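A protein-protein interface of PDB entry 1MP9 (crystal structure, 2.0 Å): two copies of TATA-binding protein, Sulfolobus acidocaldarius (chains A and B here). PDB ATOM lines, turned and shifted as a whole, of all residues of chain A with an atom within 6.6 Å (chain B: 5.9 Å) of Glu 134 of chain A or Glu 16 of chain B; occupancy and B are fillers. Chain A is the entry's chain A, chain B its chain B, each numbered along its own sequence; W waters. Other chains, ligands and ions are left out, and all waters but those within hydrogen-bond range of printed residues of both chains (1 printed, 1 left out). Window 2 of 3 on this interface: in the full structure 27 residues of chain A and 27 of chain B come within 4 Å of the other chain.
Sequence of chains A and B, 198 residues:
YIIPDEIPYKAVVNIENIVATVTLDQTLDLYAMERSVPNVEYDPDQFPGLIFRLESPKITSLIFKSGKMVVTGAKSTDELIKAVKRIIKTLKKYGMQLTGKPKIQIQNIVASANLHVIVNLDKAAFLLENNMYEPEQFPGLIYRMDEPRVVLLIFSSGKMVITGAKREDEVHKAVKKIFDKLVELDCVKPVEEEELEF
The side-chain amide nitrogen of Gln 137 of chain A sits at hydrogen-bond distance from the side-chain carboxylate of Glu 16 of chain B, at 3.4 Å.
ND2 of Asn 17 of chain B sits at hydrogen-bond distance from OG1 of Thr 72 of chain B, at 2.9 Å. The side-chain amide oxygen (OD1) of Asn 17 of chain B sits at hydrogen-bond distance from the backbone NH (N) of Gly 73 of chain B (2.7 Å). N of Glu 16 of chain B is in hydrogen-bond range of O of Val 110 of chain B, at 2.8 Å. OE2 of Glu 16 of chain B sits close to OD1 of Asn 14 of chain B (3.0 Å). N of Val 110 of chain B sits at hydrogen-bond distance from O of Asn 17 of chain B, 2.8 Å away. OE2 of Glu 16 of chain B is in hydrogen-bond range of OG of Ser 112 of chain B (2.6 Å).
Among the printed residues, pairs that only touch across the chains: Met 132 of chain A with Val 110 of chain B (3.9 Å), Glu 134 of chain A with Glu 16 of chain B (3.7 Å) and Glu 134 of chain A with Asn 17 of chain B (3.6 Å).
Tyr 133 of chain A touches none of the printed residues of chain B. Glu 134 of chain A touches just these residues of chain B: Glu 16 (3.7 Å) and Asn 17 (3.6 Å). Pro 135 of chain A touches none of the printed residues of chain B. Printed residues of chain B within 4 Å of Gln 137 of chain A: Glu 16. Printed residues of chain A within 4 Å of Glu 16 of chain B: Glu 134 and Gln 137. Of the printed residues of chain A, Val 110 of chain B touches Met 132. The nearest printed residue of chain A that does not touch Glu 16 of chain B is Glu 136 of chain A (6.6 Å).
Of the 13 printed residues of chain B, 3 touch a printed residue of chain A. Printed residues of chain A that touch a printed residue of chain B: Met 132, Glu 134 and Gln 137. Hydrophobic or aromatic side chains of chain A within 4 Å of the printed part of chain B: Met 132. Among the printed residues, 4 pairs touch across the chains. Among the printed residues, no Asp or Glu carboxylate lies within 4 Å of a Lys or Arg side-chain nitrogen of the other chain.
No position is printed for both chains.
Water W1 lies within hydrogen-bond range of the side-chain carboxylate (OE1) of Glu 134 of chain A (2.6 Å), the side-chain amide nitrogen (ND2) of Asn 17 of chain B (3.0 Å) and the backbone carbonyl oxygen (O) of Tyr 133 of chain A (3.2 Å).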
ATOM      1  N   MET A 132      14.488  -8.022 -32.140  1.00  0.00           N
ATOM      2  CA  MET A 132      13.315  -7.198 -31.963  1.00  0.00           C
ATOM      3  C   MET A 132      12.232  -7.620 -32.966  1.00  0.00           C
ATOM      4  O   MET A 132      12.495  -7.726 -34.169  1.00  0.00           O
ATOM      5  CB  MET A 132      13.599  -5.708 -32.224  1.00  0.00           C
ATOM      6  CG  MET A 132      12.288  -4.874 -32.213  1.00  0.00           C
ATOM      7  SD  MET A 132      12.501  -3.151 -32.748  1.00  0.00           S
ATOM      8  CE  MET A 132      12.273  -3.250 -34.482  1.00  0.00           C
ATOM      9  N   TYR A 133      11.036  -7.895 -32.461  1.00  0.00           N
ATOM     10  CA  TYR A 133       9.912  -8.147 -33.334  1.00  0.00           C
ATOM     11  C   TYR A 133       8.734  -7.426 -32.721  1.00  0.00           C
ATOM     12  O   TYR A 133       8.054  -7.929 -31.827  1.00  0.00           O
ATOM     13  CB  TYR A 133       9.600  -9.633 -33.562  1.00  0.00           C
ATOM     14  CG  TYR A 133       8.450  -9.801 -34.567  1.00  0.00           C
ATOM     15  CD1 TYR A 133       8.466  -9.106 -35.785  1.00  0.00           C
ATOM     16  CD2 TYR A 133       7.311 -10.571 -34.261  1.00  0.00           C
ATOM     17  CE1 TYR A 133       7.379  -9.148 -36.672  1.00  0.00           C
ATOM     18  CE2 TYR A 133       6.214 -10.629 -35.146  1.00  0.00           C
ATOM     19  CZ  TYR A 133       6.259  -9.908 -36.341  1.00  0.00           C
ATOM     20  OH  TYR A 133       5.189  -9.890 -37.206  1.00  0.00           O
ATOM     21  N   GLU A 134       8.506  -6.214 -33.204  1.00  0.00           N
ATOM     22  CA  GLU A 134       7.416  -5.363 -32.684  1.00  0.00           C
ATOM     23  C   GLU A 134       6.741  -4.871 -33.974  1.00  0.00           C
ATOM     24  O   GLU A 134       7.007  -3.770 -34.461  1.00  0.00           O
ATOM     25  CB  GLU A 134       8.053  -4.220 -31.895  1.00  0.00           C
ATOM     26  CG  GLU A 134       7.089  -3.308 -31.211  1.00  0.00           C
ATOM     27  CD  GLU A 134       6.429  -3.957 -30.029  1.00  0.00           C
ATOM     28  OE1 GLU A 134       6.795  -5.108 -29.676  1.00  0.00           O
ATOM     29  OE2 GLU A 134       5.541  -3.298 -29.451  1.00  0.00           O
ATOM     30  N   PRO A 135       5.865  -5.704 -34.544  1.00  0.00           N
ATOM     31  CA  PRO A 135       5.177  -5.370 -35.800  1.00  0.00           C
ATOM     32  C   PRO A 135       4.502  -4.022 -35.920  1.00  0.00           C
ATOM     33  O   PRO A 135       4.425  -3.472 -37.009  1.00  0.00           O
ATOM     34  CB  PRO A 135       4.238  -6.561 -36.023  1.00  0.00           C
ATOM     35  CG  PRO A 135       4.061  -7.156 -34.649  1.00  0.00           C
ATOM     36  CD  PRO A 135       5.409  -6.999 -34.006  1.00  0.00           C
ATOM     37  N   GLU A 136       4.023  -3.485 -34.817  1.00  0.00           N
ATOM     38  CA  GLU A 136       3.400  -2.173 -34.863  1.00  0.00           C
ATOM     39  C   GLU A 136       4.471  -1.088 -35.030  1.00  0.00           C
ATOM     40  O   GLU A 136       4.141   0.045 -35.351  1.00  0.00           O
ATOM     41  CB  GLU A 136       2.582  -1.911 -33.587  1.00  0.00           C
ATOM     42  CG  GLU A 136       1.266  -2.681 -33.503  1.00  0.00           C
ATOM     43  CD  GLU A 136       0.016  -1.812 -33.779  1.00  0.00           C
ATOM     44  OE1 GLU A 136      -0.134  -0.726 -33.141  1.00  0.00           O
ATOM     45  OE2 GLU A 136      -0.821  -2.224 -34.628  1.00  0.00           O
ATOM     46  N   GLN A 137       5.753  -1.413 -34.808  1.00  0.00           N
ATOM     47  CA  GLN A 137       6.814  -0.408 -34.981  1.00  0.00           C
ATOM     48  C   GLN A 137       7.647  -0.616 -36.241  1.00  0.00           C
ATOM     49  O   GLN A 137       8.075   0.355 -36.883  1.00  0.00           O
ATOM     50  CB  GLN A 137       7.769  -0.385 -33.773  1.00  0.00           C
ATOM     51  CG  GLN A 137       7.085  -0.173 -32.430  1.00  0.00           C
ATOM     52  CD  GLN A 137       6.356   1.166 -32.356  1.00  0.00           C
ATOM     53  OE1 GLN A 137       6.907   2.196 -32.719  1.00  0.00           O
ATOM     54  NE2 GLN A 137       5.119   1.145 -31.881  1.00  0.00           N
ATOM     55  N   PHE A 138       7.926  -1.872 -36.571  1.00  0.00           N
ATOM     56  CA  PHE A 138       8.726  -2.185 -37.764  1.00  0.00           C
ATOM     57  C   PHE A 138       8.155  -3.523 -38.196  1.00  0.00           C
ATOM     58  O   PHE A 138       8.007  -4.425 -37.387  1.00  0.00           O
ATOM     59  CB  PHE A 138      10.223  -2.294 -37.413  1.00  0.00           C
ATOM     60  CG  PHE A 138      11.080  -2.771 -38.553  1.00  0.00           C
ATOM     61  CD1 PHE A 138      11.372  -1.939 -39.619  1.00  0.00           C
ATOM     62  CD2 PHE A 138      11.586  -4.067 -38.564  1.00  0.00           C
ATOM     63  CE1 PHE A 138      12.157  -2.382 -40.676  1.00  0.00           C
ATOM     64  CE2 PHE A 138      12.367  -4.516 -39.620  1.00  0.00           C
ATOM     65  CZ  PHE A 138      12.654  -3.671 -40.676  1.00  0.00           C
ATOM     66  N   PRO A 139       7.855  -3.685 -39.488  1.00  0.00           N
ATOM     67  CA  PRO A 139       7.269  -4.947 -39.948  1.00  0.00           C
ATOM     68  C   PRO A 139       8.142  -6.202 -39.944  1.00  0.00           C
ATOM     69  O   PRO A 139       7.636  -7.327 -40.026  1.00  0.00           O
ATOM     70  CB  PRO A 139       6.728  -4.576 -41.321  1.00  0.00           C
ATOM     71  CG  PRO A 139       7.826  -3.631 -41.829  1.00  0.00           C
ATOM     72  CD  PRO A 139       8.114  -2.767 -40.618  1.00  0.00           C
ATOM     73  N   GLY A 140       9.440  -6.043 -39.803  1.00  0.00           N
ATOM     74  CA  GLY A 140      10.268  -7.232 -39.794  1.00  0.00           C
ATOM     75  C   GLY A 140      10.863  -7.522 -38.429  1.00  0.00           C
ATOM     76  O   GLY A 140      10.538  -6.837 -37.455  1.00  0.00           O
ATOM     77  N   LEU A 141      11.705  -8.555 -38.373  1.00  0.00           N
ATOM     78  CA  LEU A 141      12.416  -8.970 -37.168  1.00  0.00           C
ATOM     79  C   LEU A 141      13.849  -8.448 -37.347  1.00  0.00           C
ATOM     80  O   LEU A 141      14.456  -8.630 -38.410  1.00  0.00           O
ATOM     81  CB  LEU A 141      12.433 -10.502 -37.064  1.00  0.00           C
ATOM     82  CG  LEU A 141      13.089 -11.098 -35.789  1.00  0.00           C
ATOM     83  CD1 LEU A 141      12.427 -12.413 -35.419  1.00  0.00           C
ATOM     84  CD2 LEU A 141      14.562 -11.302 -35.988  1.00  0.00           C
ATOM     85  N   ASN B  14       8.979   6.846 -25.452  1.00  0.00           N
ATOM     86  CA  ASN B  14       7.834   6.050 -25.066  1.00  0.00           C
ATOM     87  C   ASN B  14       8.217   4.570 -25.106  1.00  0.00           C
ATOM     88  O   ASN B  14       8.788   4.093 -26.092  1.00  0.00           O
ATOM     89  CB  ASN B  14       6.651   6.266 -26.005  1.00  0.00           C
ATOM     90  CG  ASN B  14       5.401   5.559 -25.510  1.00  0.00           C
ATOM     91  OD1 ASN B  14       4.887   4.646 -26.152  1.00  0.00           O
ATOM     92  ND2 ASN B  14       4.921   5.967 -24.343  1.00  0.00           N
ATOM     93  N   ILE B  15       7.929   3.851 -24.028  1.00  0.00           N
ATOM     94  CA  ILE B  15       8.228   2.420 -24.012  1.00  0.00           C
ATOM     95  C   ILE B  15       7.070   1.716 -24.716  1.00  0.00           C
ATOM     96  O   ILE B  15       5.913   1.902 -24.353  1.00  0.00           O
ATOM     97  CB  ILE B  15       8.381   1.917 -22.604  1.00  0.00           C
ATOM     98  CG1 ILE B  15       9.644   2.562 -22.008  1.00  0.00           C
ATOM     99  CG2 ILE B  15       8.489   0.361 -22.603  1.00  0.00           C
ATOM    100  CD1 ILE B  15       9.952   2.100 -20.575  1.00  0.00           C
ATOM    101  N   GLU B  16       7.394   0.949 -25.747  1.00  0.00           N
ATOM    102  CA  GLU B  16       6.401   0.234 -26.541  1.00  0.00           C
ATOM    103  C   GLU B  16       6.186  -1.182 -26.056  1.00  0.00           C
ATOM    104  O   GLU B  16       5.078  -1.697 -26.144  1.00  0.00           O
ATOM    105  CB  GLU B  16       6.849   0.209 -28.007  1.00  0.00           C
ATOM    106  CG  GLU B  16       7.025   1.627 -28.625  1.00  0.00           C
ATOM    107  CD  GLU B  16       5.734   2.436 -28.699  1.00  0.00           C
ATOM    108  OE1 GLU B  16       4.657   1.842 -28.603  1.00  0.00           O
ATOM    109  OE2 GLU B  16       5.790   3.672 -28.865  1.00  0.00           O
ATOM    110  N   ASN B  17       7.248  -1.825 -25.566  1.00  0.00           N
ATOM    111  CA  ASN B  17       7.140  -3.204 -25.074  1.00  0.00           C
ATOM    112  C   ASN B  17       8.383  -3.606 -24.290  1.00  0.00           C
ATOM    113  O   ASN B  17       9.484  -3.134 -24.556  1.00  0.00           O
ATOM    114  CB  ASN B  17       7.016  -4.201 -26.238  1.00  0.00           C
ATOM    115  CG  ASN B  17       6.601  -5.586 -25.765  1.00  0.00           C
ATOM    116  OD1 ASN B  17       5.719  -5.702 -24.923  1.00  0.00           O
ATOM    117  ND2 ASN B  17       7.220  -6.645 -26.318  1.00  0.00           N
ATOM    118  N   ILE B  18       8.196  -4.479 -23.325  1.00  0.00           N
ATOM    119  CA  ILE B  18       9.305  -4.985 -22.562  1.00  0.00           C
ATOM    120  C   ILE B  18       9.162  -6.489 -22.655  1.00  0.00           C
ATOM    121  O   ILE B  18       8.035  -7.017 -22.616  1.00  0.00           O
ATOM    122  CB  ILE B  18       9.220  -4.580 -21.083  1.00  0.00           C
ATOM    123  CG1 ILE B  18       9.394  -3.065 -20.954  1.00  0.00           C
ATOM    124  CG2 ILE B  18      10.262  -5.342 -20.279  1.00  0.00           C
ATOM    125  CD1 ILE B  18       8.820  -2.518 -19.650  1.00  0.00           C
ATOM    126  N   THR B  72       5.747 -10.926 -22.303  1.00  0.00           N
ATOM    127  CA  THR B  72       5.843  -9.826 -23.260  1.00  0.00           C
ATOM    128  C   THR B  72       4.528  -9.056 -23.258  1.00  0.00           C
ATOM    129  O   THR B  72       3.480  -9.618 -22.934  1.00  0.00           O
ATOM    130  CB  THR B  72       6.091 -10.387 -24.684  1.00  0.00           C
ATOM    131  OG1 THR B  72       6.225  -9.317 -25.616  1.00  0.00           O
ATOM    132  CG2 THR B  72       4.904 -11.264 -25.112  1.00  0.00           C
ATOM    133  N   GLY B  73       4.587  -7.776 -23.614  1.00  0.00           N
ATOM    134  CA  GLY B  73       3.382  -6.966 -23.672  1.00  0.00           C
ATOM    135  C   GLY B  73       3.359  -5.756 -22.762  1.00  0.00           C
ATOM    136  O   GLY B  73       2.779  -4.724 -23.111  1.00  0.00           O
ATOM    137  N   ALA B  74       4.013  -5.851 -21.610  1.00  0.00           N
ATOM    138  CA  ALA B  74       4.017  -4.741 -20.658  1.00  0.00           C
ATOM    139  C   ALA B  74       4.716  -3.496 -21.218  1.00  0.00           C
ATOM    140  O   ALA B  74       5.709  -3.613 -21.958  1.00  0.00           O
ATOM    141  CB  ALA B  74       4.685  -5.183 -19.356  1.00  0.00           C
ATOM    142  N   LYS B  75       4.206  -2.310 -20.878  1.00  0.00           N
ATOM    143  CA  LYS B  75       4.831  -1.077 -21.359  1.00  0.00           C
ATOM    144  C   LYS B  75       5.523  -0.309 -20.257  1.00  0.00           C
ATOM    145  O   LYS B  75       5.966   0.797 -20.473  1.00  0.00           O
ATOM    146  CB  LYS B  75       3.817  -0.187 -22.057  1.00  0.00           C
ATOM    147  CG  LYS B  75       3.386  -0.752 -23.405  1.00  0.00           C
ATOM    148  CD  LYS B  75       2.150  -0.077 -23.950  1.00  0.00           C
ATOM    149  CE  LYS B  75       1.620  -0.824 -25.161  1.00  0.00           C
ATOM    150  NZ  LYS B  75       0.447  -0.130 -25.819  1.00  0.00           N
ATOM    151  N   ILE B 109      13.985  -4.094 -24.200  1.00  0.00           N
ATOM    152  CA  ILE B 109      13.006  -3.053 -24.104  1.00  0.00           C
ATOM    153  C   ILE B 109      12.895  -2.492 -25.507  1.00  0.00           C
ATOM    154  O   ILE B 109      13.908  -2.267 -26.157  1.00  0.00           O
ATOM    155  CB  ILE B 109      13.447  -1.903 -23.169  1.00  0.00           C
ATOM    156  CG1 ILE B 109      13.656  -2.435 -21.741  1.00  0.00           C
ATOM    157  CG2 ILE B 109      12.332  -0.839 -23.138  1.00  0.00           C
ATOM    158  CD1 ILE B 109      14.190  -1.407 -20.771  1.00  0.00           C
ATOM    159  N   VAL B 110      11.677  -2.316 -26.003  1.00  0.00           N
ATOM    160  CA  VAL B 110      11.545  -1.705 -27.319  1.00  0.00           C
ATOM    161  C   VAL B 110      10.909  -0.365 -27.054  1.00  0.00           C
ATOM    162  O   VAL B 110       9.869  -0.291 -26.417  1.00  0.00           O
ATOM    163  CB  VAL B 110      10.629  -2.485 -28.282  1.00  0.00           C
ATOM    164  CG1 VAL B 110      10.475  -1.635 -29.598  1.00  0.00           C
ATOM    165  CG2 VAL B 110      11.237  -3.852 -28.627  1.00  0.00           C
ATOM    166  N   ALA B 111      11.560   0.704 -27.492  1.00  0.00           N
ATOM    167  CA  ALA B 111      11.020   2.046 -27.289  1.00  0.00           C
ATOM    168  C   ALA B 111      10.977   2.808 -28.580  1.00  0.00           C
ATOM    169  O   ALA B 111      11.633   2.436 -29.553  1.00  0.00           O
ATOM    170  CB  ALA B 111      11.867   2.833 -26.296  1.00  0.00           C
ATOM    171  N   SER B 112      10.174   3.867 -28.581  1.00  0.00           N
ATOM    172  CA  SER B 112      10.074   4.780 -29.711  1.00  0.00           C
ATOM    173  C   SER B 112      10.414   6.132 -29.100  1.00  0.00           C
ATOM    174  O   SER B 112      10.375   6.294 -27.865  1.00  0.00           O
ATOM    175  CB  SER B 112       8.641   4.867 -30.235  1.00  0.00           C
ATOM    176  OG  SER B 112       7.760   5.336 -29.216  1.00  0.00           O
HETATM  177  O   HOH W   1       8.695  -6.790 -28.939  1.00  0.00           O
